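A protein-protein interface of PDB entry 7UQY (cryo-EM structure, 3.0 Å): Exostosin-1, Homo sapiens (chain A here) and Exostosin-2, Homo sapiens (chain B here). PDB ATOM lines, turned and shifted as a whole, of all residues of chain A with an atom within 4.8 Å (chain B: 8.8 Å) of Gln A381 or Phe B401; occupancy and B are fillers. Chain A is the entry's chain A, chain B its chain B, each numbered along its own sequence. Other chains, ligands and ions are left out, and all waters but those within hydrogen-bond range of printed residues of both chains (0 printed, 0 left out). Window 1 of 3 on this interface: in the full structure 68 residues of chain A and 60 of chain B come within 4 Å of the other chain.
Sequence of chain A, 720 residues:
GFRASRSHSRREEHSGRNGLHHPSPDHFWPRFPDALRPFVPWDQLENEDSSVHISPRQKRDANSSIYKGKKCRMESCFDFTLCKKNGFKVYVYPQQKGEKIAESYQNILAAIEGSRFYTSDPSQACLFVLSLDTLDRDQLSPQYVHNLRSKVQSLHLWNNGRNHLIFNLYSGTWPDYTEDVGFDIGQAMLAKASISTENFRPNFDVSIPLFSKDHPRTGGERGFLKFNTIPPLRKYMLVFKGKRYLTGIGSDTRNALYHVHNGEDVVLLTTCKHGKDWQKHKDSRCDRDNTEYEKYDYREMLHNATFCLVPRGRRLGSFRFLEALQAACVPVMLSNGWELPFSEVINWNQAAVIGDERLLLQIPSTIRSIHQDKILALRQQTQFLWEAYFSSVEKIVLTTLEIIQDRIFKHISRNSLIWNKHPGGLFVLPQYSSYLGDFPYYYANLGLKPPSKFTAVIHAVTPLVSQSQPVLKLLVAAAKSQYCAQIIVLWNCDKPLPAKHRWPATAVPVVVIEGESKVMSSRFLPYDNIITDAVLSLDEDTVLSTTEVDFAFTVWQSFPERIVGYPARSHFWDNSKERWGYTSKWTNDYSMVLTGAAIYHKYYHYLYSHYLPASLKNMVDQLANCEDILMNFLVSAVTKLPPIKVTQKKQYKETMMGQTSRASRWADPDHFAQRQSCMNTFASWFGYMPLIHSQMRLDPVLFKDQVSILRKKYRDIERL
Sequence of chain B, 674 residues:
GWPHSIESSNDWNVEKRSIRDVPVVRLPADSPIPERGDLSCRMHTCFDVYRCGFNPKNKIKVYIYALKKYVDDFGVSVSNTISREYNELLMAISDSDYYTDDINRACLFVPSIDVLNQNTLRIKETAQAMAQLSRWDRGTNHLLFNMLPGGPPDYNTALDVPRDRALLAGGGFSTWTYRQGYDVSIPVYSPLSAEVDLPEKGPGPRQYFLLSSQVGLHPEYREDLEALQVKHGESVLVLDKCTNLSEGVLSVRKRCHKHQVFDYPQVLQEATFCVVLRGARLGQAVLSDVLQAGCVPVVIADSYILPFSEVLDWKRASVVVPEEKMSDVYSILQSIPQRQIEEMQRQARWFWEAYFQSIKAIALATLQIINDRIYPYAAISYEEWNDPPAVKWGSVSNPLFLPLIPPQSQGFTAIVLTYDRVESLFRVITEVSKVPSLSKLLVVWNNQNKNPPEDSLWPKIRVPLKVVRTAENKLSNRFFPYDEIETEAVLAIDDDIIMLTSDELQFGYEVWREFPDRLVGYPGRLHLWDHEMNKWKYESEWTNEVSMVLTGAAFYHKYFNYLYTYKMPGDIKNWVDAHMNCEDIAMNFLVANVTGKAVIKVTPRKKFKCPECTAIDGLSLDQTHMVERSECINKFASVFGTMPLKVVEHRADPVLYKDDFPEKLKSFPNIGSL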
ATOM      1  N   GLN A 350     -19.227 -20.204  19.780  1.00  0.00           N
ATOM      2  CA  GLN A 350     -18.700 -19.031  20.458  1.00  0.00           C
ATOM      3  C   GLN A 350     -19.757 -18.265  21.239  1.00  0.00           C
ATOM      4  O   GLN A 350     -19.402 -17.479  22.122  1.00  0.00           O
ATOM      5  CB  GLN A 350     -18.047 -18.092  19.437  1.00  0.00           C
ATOM      6  CG  GLN A 350     -17.083 -17.080  20.023  1.00  0.00           C
ATOM      7  CD  GLN A 350     -16.424 -16.231  18.956  1.00  0.00           C
ATOM      8  OE1 GLN A 350     -16.780 -16.306  17.781  1.00  0.00           O
ATOM      9  NE2 GLN A 350     -15.457 -15.416  19.361  1.00  0.00           N
ATOM     10  N   ALA A 351     -21.041 -18.477  20.945  1.00  0.00           N
ATOM     11  CA  ALA A 351     -22.120 -17.770  21.617  1.00  0.00           C
ATOM     12  C   ALA A 351     -23.126 -18.687  22.291  1.00  0.00           C
ATOM     13  O   ALA A 351     -24.048 -18.188  22.946  1.00  0.00           O
ATOM     14  CB  ALA A 351     -22.863 -16.862  20.629  1.00  0.00           C
ATOM     15  N   ALA A 377     -17.231 -15.267  28.026  1.00  0.00           N
ATOM     16  CA  ALA A 377     -17.119 -15.107  26.580  1.00  0.00           C
ATOM     17  C   ALA A 377     -18.415 -15.486  25.875  1.00  0.00           C
ATOM     18  O   ALA A 377     -18.864 -14.779  24.967  1.00  0.00           O
ATOM     19  CB  ALA A 377     -15.954 -15.941  26.049  1.00  0.00           C
ATOM     20  N   LEU A 378     -19.030 -16.601  26.280  1.00  0.00           N
ATOM     21  CA  LEU A 378     -20.275 -17.033  25.655  1.00  0.00           C
ATOM     22  C   LEU A 378     -21.386 -16.017  25.874  1.00  0.00           C
ATOM     23  O   LEU A 378     -22.143 -15.707  24.949  1.00  0.00           O
ATOM     24  CB  LEU A 378     -20.694 -18.399  26.196  1.00  0.00           C
ATOM     25  CG  LEU A 378     -19.808 -19.608  25.896  1.00  0.00           C
ATOM     26  CD1 LEU A 378     -20.578 -20.892  26.121  1.00  0.00           C
ATOM     27  CD2 LEU A 378     -19.255 -19.558  24.485  1.00  0.00           C
ATOM     28  N   ARG A 379     -21.497 -15.482  27.093  1.00  0.00           N
ATOM     29  CA  ARG A 379     -22.521 -14.486  27.386  1.00  0.00           C
ATOM     30  C   ARG A 379     -22.329 -13.236  26.538  1.00  0.00           C
ATOM     31  O   ARG A 379     -23.283 -12.718  25.936  1.00  0.00           O
ATOM     32  CB  ARG A 379     -22.478 -14.142  28.876  1.00  0.00           C
ATOM     33  CG  ARG A 379     -23.785 -13.653  29.465  1.00  0.00           C
ATOM     34  CD  ARG A 379     -23.795 -13.839  30.974  1.00  0.00           C
ATOM     35  NE  ARG A 379     -22.698 -13.130  31.622  1.00  0.00           N
ATOM     36  CZ  ARG A 379     -22.850 -12.225  32.579  1.00  0.00           C
ATOM     37  NH1 ARG A 379     -24.045 -11.903  33.043  1.00  0.00           N
ATOM     38  NH2 ARG A 379     -21.773 -11.631  33.086  1.00  0.00           N
ATOM     39  N   GLN A 380     -21.091 -12.743  26.468  1.00  0.00           N
ATOM     40  CA  GLN A 380     -20.830 -11.526  25.707  1.00  0.00           C
ATOM     41  C   GLN A 380     -21.086 -11.741  24.220  1.00  0.00           C
ATOM     42  O   GLN A 380     -21.662 -10.876  23.545  1.00  0.00           O
ATOM     43  CB  GLN A 380     -19.396 -11.070  25.951  1.00  0.00           C
ATOM     44  CG  GLN A 380     -19.186 -10.461  27.319  1.00  0.00           C
ATOM     45  CD  GLN A 380     -17.729 -10.245  27.641  1.00  0.00           C
ATOM     46  OE1 GLN A 380     -17.258  -9.112  27.686  1.00  0.00           O
ATOM     47  NE2 GLN A 380     -17.003 -11.333  27.863  1.00  0.00           N
ATOM     48  N   GLN A 381     -20.673 -12.896  23.693  1.00  0.00           N
ATOM     49  CA  GLN A 381     -20.891 -13.193  22.282  1.00  0.00           C
ATOM     50  C   GLN A 381     -22.374 -13.356  21.980  1.00  0.00           C
ATOM     51  O   GLN A 381     -22.841 -12.962  20.905  1.00  0.00           O
ATOM     52  CB  GLN A 381     -20.111 -14.450  21.897  1.00  0.00           C
ATOM     53  CG  GLN A 381     -20.088 -14.770  20.415  1.00  0.00           C
ATOM     54  CD  GLN A 381     -19.434 -13.683  19.591  1.00  0.00           C
ATOM     55  OE1 GLN A 381     -20.107 -12.947  18.875  1.00  0.00           O
ATOM     56  NE2 GLN A 381     -18.116 -13.577  19.691  1.00  0.00           N
ATOM     57  N   THR A 382     -23.130 -13.936  22.915  1.00  0.00           N
ATOM     58  CA  THR A 382     -24.576 -14.044  22.759  1.00  0.00           C
ATOM     59  C   THR A 382     -25.216 -12.667  22.667  1.00  0.00           C
ATOM     60  O   THR A 382     -26.061 -12.413  21.797  1.00  0.00           O
ATOM     61  CB  THR A 382     -25.156 -14.833  23.935  1.00  0.00           C
ATOM     62  OG1 THR A 382     -24.599 -16.152  23.951  1.00  0.00           O
ATOM     63  CG2 THR A 382     -26.658 -14.923  23.836  1.00  0.00           C
ATOM     64  N   GLN A 383     -24.809 -11.757  23.554  1.00  0.00           N
ATOM     65  CA  GLN A 383     -25.329 -10.395  23.497  1.00  0.00           C
ATOM     66  C   GLN A 383     -24.990  -9.729  22.170  1.00  0.00           C
ATOM     67  O   GLN A 383     -25.848  -9.084  21.552  1.00  0.00           O
ATOM     68  CB  GLN A 383     -24.782  -9.572  24.662  1.00  0.00           C
ATOM     69  CG  GLN A 383     -25.564  -9.725  25.948  1.00  0.00           C
ATOM     70  CD  GLN A 383     -26.981  -9.215  25.821  1.00  0.00           C
ATOM     71  OE1 GLN A 383     -27.925  -9.995  25.706  1.00  0.00           O
ATOM     72  NE2 GLN A 383     -27.139  -7.898  25.835  1.00  0.00           N
ATOM     73  N   PHE A 384     -23.744  -9.881  21.714  1.00  0.00           N
ATOM     74  CA  PHE A 384     -23.342  -9.252  20.459  1.00  0.00           C
ATOM     75  C   PHE A 384     -24.134  -9.807  19.283  1.00  0.00           C
ATOM     76  O   PHE A 384     -24.585  -9.052  18.413  1.00  0.00           O
ATOM     77  CB  PHE A 384     -21.844  -9.437  20.225  1.00  0.00           C
ATOM     78  CG  PHE A 384     -21.427  -9.205  18.802  1.00  0.00           C
ATOM     79  CD1 PHE A 384     -21.371  -7.923  18.285  1.00  0.00           C
ATOM     80  CD2 PHE A 384     -21.105 -10.268  17.977  1.00  0.00           C
ATOM     81  CE1 PHE A 384     -20.994  -7.707  16.977  1.00  0.00           C
ATOM     82  CE2 PHE A 384     -20.728 -10.058  16.669  1.00  0.00           C
ATOM     83  CZ  PHE A 384     -20.673  -8.776  16.168  1.00  0.00           C
ATOM     84  N   LEU A 385     -24.310 -11.131  19.234  1.00  0.00           N
ATOM     85  CA  LEU A 385     -25.064 -11.734  18.139  1.00  0.00           C
ATOM     86  C   LEU A 385     -26.504 -11.251  18.126  1.00  0.00           C
ATOM     87  O   LEU A 385     -27.037 -10.896  17.067  1.00  0.00           O
ATOM     88  CB  LEU A 385     -25.022 -13.258  18.236  1.00  0.00           C
ATOM     89  CG  LEU A 385     -23.722 -13.969  17.871  1.00  0.00           C
ATOM     90  CD1 LEU A 385     -24.018 -15.414  17.537  1.00  0.00           C
ATOM     91  CD2 LEU A 385     -23.039 -13.278  16.704  1.00  0.00           C
ATOM     92  N   ASN A 420     -18.234 -13.144  13.049  1.00  0.00           N
ATOM     93  CA  ASN A 420     -18.204 -13.526  14.455  1.00  0.00           C
ATOM     94  C   ASN A 420     -17.405 -12.550  15.311  1.00  0.00           C
ATOM     95  O   ASN A 420     -16.807 -12.950  16.314  1.00  0.00           O
ATOM     96  CB  ASN A 420     -17.650 -14.939  14.602  1.00  0.00           C
ATOM     97  CG  ASN A 420     -18.365 -15.934  13.719  1.00  0.00           C
ATOM     98  OD1 ASN A 420     -19.352 -16.540  14.125  1.00  0.00           O
ATOM     99  ND2 ASN A 420     -17.867 -16.110  12.503  1.00  0.00           N
ATOM    100  N   GLU B 383      -8.878 -18.523  16.450  1.00  0.00           N
ATOM    101  CA  GLU B 383      -7.500 -18.057  16.344  1.00  0.00           C
ATOM    102  C   GLU B 383      -6.513 -19.199  16.541  1.00  0.00           C
ATOM    103  O   GLU B 383      -5.543 -19.325  15.788  1.00  0.00           O
ATOM    104  CB  GLU B 383      -7.228 -16.936  17.352  1.00  0.00           C
ATOM    105  CG  GLU B 383      -8.251 -15.797  17.378  1.00  0.00           C
ATOM    106  CD  GLU B 383      -9.564 -16.175  18.039  1.00  0.00           C
ATOM    107  OE1 GLU B 383      -9.551 -17.052  18.928  1.00  0.00           O
ATOM    108  OE2 GLU B 383     -10.606 -15.596  17.668  1.00  0.00           O
ATOM    109  N   SER B 397      -7.300 -10.502  21.833  1.00  0.00           N
ATOM    110  CA  SER B 397      -8.478 -11.262  22.260  1.00  0.00           C
ATOM    111  C   SER B 397      -8.970 -10.786  23.632  1.00  0.00           C
ATOM    112  O   SER B 397      -8.935 -11.507  24.631  1.00  0.00           O
ATOM    113  CB  SER B 397      -8.186 -12.768  22.265  1.00  0.00           C
ATOM    114  OG  SER B 397      -9.319 -13.502  22.695  1.00  0.00           O
ATOM    115  N   ASN B 398      -9.408  -9.513  23.707  1.00  0.00           N
ATOM    116  CA  ASN B 398      -9.846  -8.839  24.973  1.00  0.00           C
ATOM    117  C   ASN B 398     -11.025  -9.543  25.614  1.00  0.00           C
ATOM    118  O   ASN B 398     -12.032  -9.758  24.913  1.00  0.00           O
ATOM    119  CB  ASN B 398     -10.204  -7.376  24.728  1.00  0.00           C
ATOM    120  CG  ASN B 398     -10.800  -6.638  25.904  1.00  0.00           C
ATOM    121  OD1 ASN B 398     -10.401  -6.828  27.045  1.00  0.00           O
ATOM    122  ND2 ASN B 398     -11.728  -5.741  25.622  1.00  0.00           N
ATOM    123  N   PRO B 399     -10.962  -9.903  26.911  1.00  0.00           N
ATOM    124  CA  PRO B 399     -12.030 -10.694  27.525  1.00  0.00           C
ATOM    125  C   PRO B 399     -13.338  -9.917  27.711  1.00  0.00           C
ATOM    126  O   PRO B 399     -14.343 -10.553  27.818  1.00  0.00           O
ATOM    127  CB  PRO B 399     -11.375 -11.096  28.842  1.00  0.00           C
ATOM    128  CG  PRO B 399     -10.434  -9.967  29.153  1.00  0.00           C
ATOM    129  CD  PRO B 399      -9.831  -9.663  27.806  1.00  0.00           C
ATOM    130  N   LEU B 400     -13.287  -8.588  27.747  1.00  0.00           N
ATOM    131  CA  LEU B 400     -14.490  -7.731  27.883  1.00  0.00           C
ATOM    132  C   LEU B 400     -14.754  -7.082  26.526  1.00  0.00           C
ATOM    133  O   LEU B 400     -14.389  -5.922  26.345  1.00  0.00           O
ATOM    134  CB  LEU B 400     -14.232  -6.713  28.995  1.00  0.00           C
ATOM    135  CG  LEU B 400     -13.826  -7.316  30.338  1.00  0.00           C
ATOM    136  CD1 LEU B 400     -13.517  -6.235  31.358  1.00  0.00           C
ATOM    137  CD2 LEU B 400     -14.901  -8.253  30.864  1.00  0.00           C
ATOM    138  N   PHE B 401     -15.399  -7.813  25.612  1.00  0.00           N
ATOM    139  CA  PHE B 401     -15.534  -7.285  24.227  1.00  0.00           C
ATOM    140  C   PHE B 401     -16.925  -6.716  23.913  1.00  0.00           C
ATOM    141  O   PHE B 401     -17.152  -6.415  22.724  1.00  0.00           O
ATOM    142  CB  PHE B 401     -15.120  -8.355  23.208  1.00  0.00           C
ATOM    143  CG  PHE B 401     -15.788  -9.701  23.349  1.00  0.00           C
ATOM    144  CD1 PHE B 401     -16.933 -10.004  22.630  1.00  0.00           C
ATOM    145  CD2 PHE B 401     -15.255 -10.677  24.176  1.00  0.00           C
ATOM    146  CE1 PHE B 401     -17.538 -11.245  22.748  1.00  0.00           C
ATOM    147  CE2 PHE B 401     -15.862 -11.917  24.296  1.00  0.00           C
ATOM    148  CZ  PHE B 401     -17.000 -12.200  23.579  1.00  0.00           C
ATOM    149  N   LEU B 402     -17.822  -6.556  24.895  1.00  0.00           N
ATOM    150  CA  LEU B 402     -19.095  -5.911  24.510  1.00  0.00           C
ATOM    151  C   LEU B 402     -18.978  -4.424  24.732  1.00  0.00           C
ATOM    152  O   LEU B 402     -18.519  -4.036  25.799  1.00  0.00           O
ATOM    153  CB  LEU B 402     -20.238  -6.468  25.340  1.00  0.00           C
ATOM    154  CG  LEU B 402     -20.969  -7.666  24.754  1.00  0.00           C
ATOM    155  CD1 LEU B 402     -21.962  -8.188  25.774  1.00  0.00           C
ATOM    156  CD2 LEU B 402     -21.678  -7.277  23.469  1.00  0.00           C
ATOM    157  N   PRO B 403     -19.369  -3.577  23.778  1.00  0.00           N
ATOM    158  CA  PRO B 403     -19.351  -2.150  24.042  1.00  0.00           C
ATOM    159  C   PRO B 403     -20.545  -1.738  24.928  1.00  0.00           C
ATOM    160  O   PRO B 403     -21.388  -1.002  24.447  1.00  0.00           O
ATOM    161  CB  PRO B 403     -19.408  -1.580  22.624  1.00  0.00           C
ATOM    162  CG  PRO B 403     -20.175  -2.611  21.827  1.00  0.00           C
ATOM    163  CD  PRO B 403     -19.797  -3.942  22.434  1.00  0.00           C
ATOM    164  N   LEU B 404     -20.588  -2.194  26.195  1.00  0.00           N
ATOM    165  CA  LEU B 404     -21.711  -1.884  27.117  1.00  0.00           C
ATOM    166  C   LEU B 404     -21.344  -0.736  28.029  1.00  0.00           C
ATOM    167  O   LEU B 404     -20.198  -0.703  28.479  1.00  0.00           O
ATOM    168  CB  LEU B 404     -22.014  -3.110  27.963  1.00  0.00           C
ATOM    169  CG  LEU B 404     -22.709  -4.250  27.232  1.00  0.00           C
ATOM    170  CD1 LEU B 404     -22.760  -5.480  28.112  1.00  0.00           C
ATOM    171  CD2 LEU B 404     -24.108  -3.842  26.800  1.00  0.00           C
ATOM    172  N   PRO B 516     -15.339   0.226  30.550  1.00  0.00           N
ATOM    173  CA  PRO B 516     -15.327  -0.831  31.568  1.00  0.00           C
ATOM    174  C   PRO B 516     -14.290  -1.917  31.328  1.00  0.00           C
ATOM    175  O   PRO B 516     -14.006  -2.687  32.255  1.00  0.00           O
ATOM    176  CB  PRO B 516     -16.745  -1.408  31.480  1.00  0.00           C
ATOM    177  CG  PRO B 516     -17.135  -1.187  30.063  1.00  0.00           C
ATOM    178  CD  PRO B 516     -16.497   0.112  29.647  1.00  0.00           C
ATOM    179  N   ASP B 517     -13.717  -2.004  30.128  1.00  0.00           N
ATOM    180  CA  ASP B 517     -12.826  -3.097  29.767  1.00  0.00           C
ATOM    181  C   ASP B 517     -11.354  -2.793  30.007  1.00  0.00           C
ATOM    182  O   ASP B 517     -10.514  -3.669  29.785  1.00  0.00           O
ATOM    183  CB  ASP B 517     -13.039  -3.481  28.297  1.00  0.00           C
ATOM    184  CG  ASP B 517     -12.753  -2.334  27.344  1.00  0.00           C
ATOM    185  OD1 ASP B 517     -12.499  -1.206  27.814  1.00  0.00           O
ATOM    186  OD2 ASP B 517     -12.784  -2.565  26.117  1.00  0.00           O
ATOM    187  N   THR B 595      -6.028  -6.913  27.728  1.00  0.00           N
ATOM    188  CA  THR B 595      -6.943  -6.078  26.967  1.00  0.00           C
ATOM    189  C   THR B 595      -6.313  -5.495  25.712  1.00  0.00           C
ATOM    190  O   THR B 595      -7.044  -5.115  24.791  1.00  0.00           O
ATOM    191  CB  THR B 595      -7.474  -4.934  27.837  1.00  0.00           C
ATOM    192  OG1 THR B 595      -6.452  -3.945  28.006  1.00  0.00           O
ATOM    193  CG2 THR B 595      -7.900  -5.456  29.196  1.00  0.00           C
ATOM    194  N   LYS B 597      -5.174  -2.690  25.328  1.00  0.00           N
ATOM    195  CA  LYS B 597      -5.620  -1.312  25.231  1.00  0.00           C
ATOM    196  C   LYS B 597      -4.778  -0.428  26.139  1.00  0.00           C
ATOM    197  O   LYS B 597      -4.024  -0.903  26.992  1.00  0.00           O
ATOM    198  CB  LYS B 597      -7.105  -1.189  25.588  1.00  0.00           C
ATOM    199  CG  LYS B 597      -8.037  -1.819  24.565  1.00  0.00           C
ATOM    200  CD  LYS B 597      -9.493  -1.640  24.955  1.00  0.00           C
ATOM    201  CE  LYS B 597     -10.419  -2.199  23.888  1.00  0.00           C
ATOM    202  NZ  LYS B 597     -10.313  -3.679  23.779  1.00  0.00           N
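The side-chain amide nitrogen of Gln A380 is in hydrogen-bond range of the backbone carbonyl oxygen of Pro B399, at 2.8 Å.
N of Phe B401 lies within hydrogen-bond range of OE1 of Gln A380.
NE2 of Gln A381 lies close to NE2 of Gln A350, at 3.2 Å.
The side-chain amide nitrogen (ND2) of Asn B398 sits at hydrogen-bond distance from the backbone carbonyl oxygen (O) of Leu B400, at 2.8 Å.
Among the printed residues, pairs that only touch across the chains: Ala A377 with Phe B401, Gln A380 with Leu B400, Gln A380 with Leu B402, Gln A381 with Phe B401, Gln A383 with Leu B402 and Phe A384 with Leu B402.
Gln A381 touches one residue of chain B.
Of chain A, only Ala A377 (3.5 Å), Gln A380 (3.1 Å) and Gln A381 (3.7 Å) come within 4 Å of Phe B401.
Of chain B, only Pro B399 (2.8 Å), Leu B400 (3.1 Å), Phe B401 (3.1 Å) and Leu B402 (3.5 Å) come within 4 Å of Gln A380.
Of the printed residues of chain A, Leu B400 touches Gln A380 (3.1 Å).
Of the printed residues of chain A, Pro B399 touches Gln A380.
Of the printed residues of chain B, Phe A384 touches Leu B402 (3.8 Å).
Of the printed residues of chain B, Gln A383 touches Leu B402 (3.3 Å).
Of the printed residues of chain B, Ala A377 touches Phe B401 (3.5 Å).
Pro B403 touches none of the printed residues of chain A.
Thr B595 touches none of the printed residues of chain A.
The nearest residue of chain B that does not touch Gln A381 is Leu B402 (5.3 Å).
The nearest printed residue of chain B that does not touch Ala A377 is Pro B399 (5.5 Å).
Of the 13 printed residues of chain B, 4 touch a printed residue of chain A.
Printed residues of chain B that touch a printed residue of chain A: Pro B399, Leu B400, Phe B401 and Leu B402.
Hydrophobic or aromatic side chains of chain B that line the printed part of chain A: Phe B401 and Leu B402.
Of the 12 printed residues of chain A, 5 touch a printed residue of chain B.
Hydrophobic or aromatic side chains of chain A that line the printed part of chain B: Phe A384.
Along chain A the printed residues that touch a printed residue of chain B span positions 377 to 384.
Among the printed residues, no Asp or Glu carboxylate lies within 4 Å of a Lys or Arg side-chain nitrogen of the other chain.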
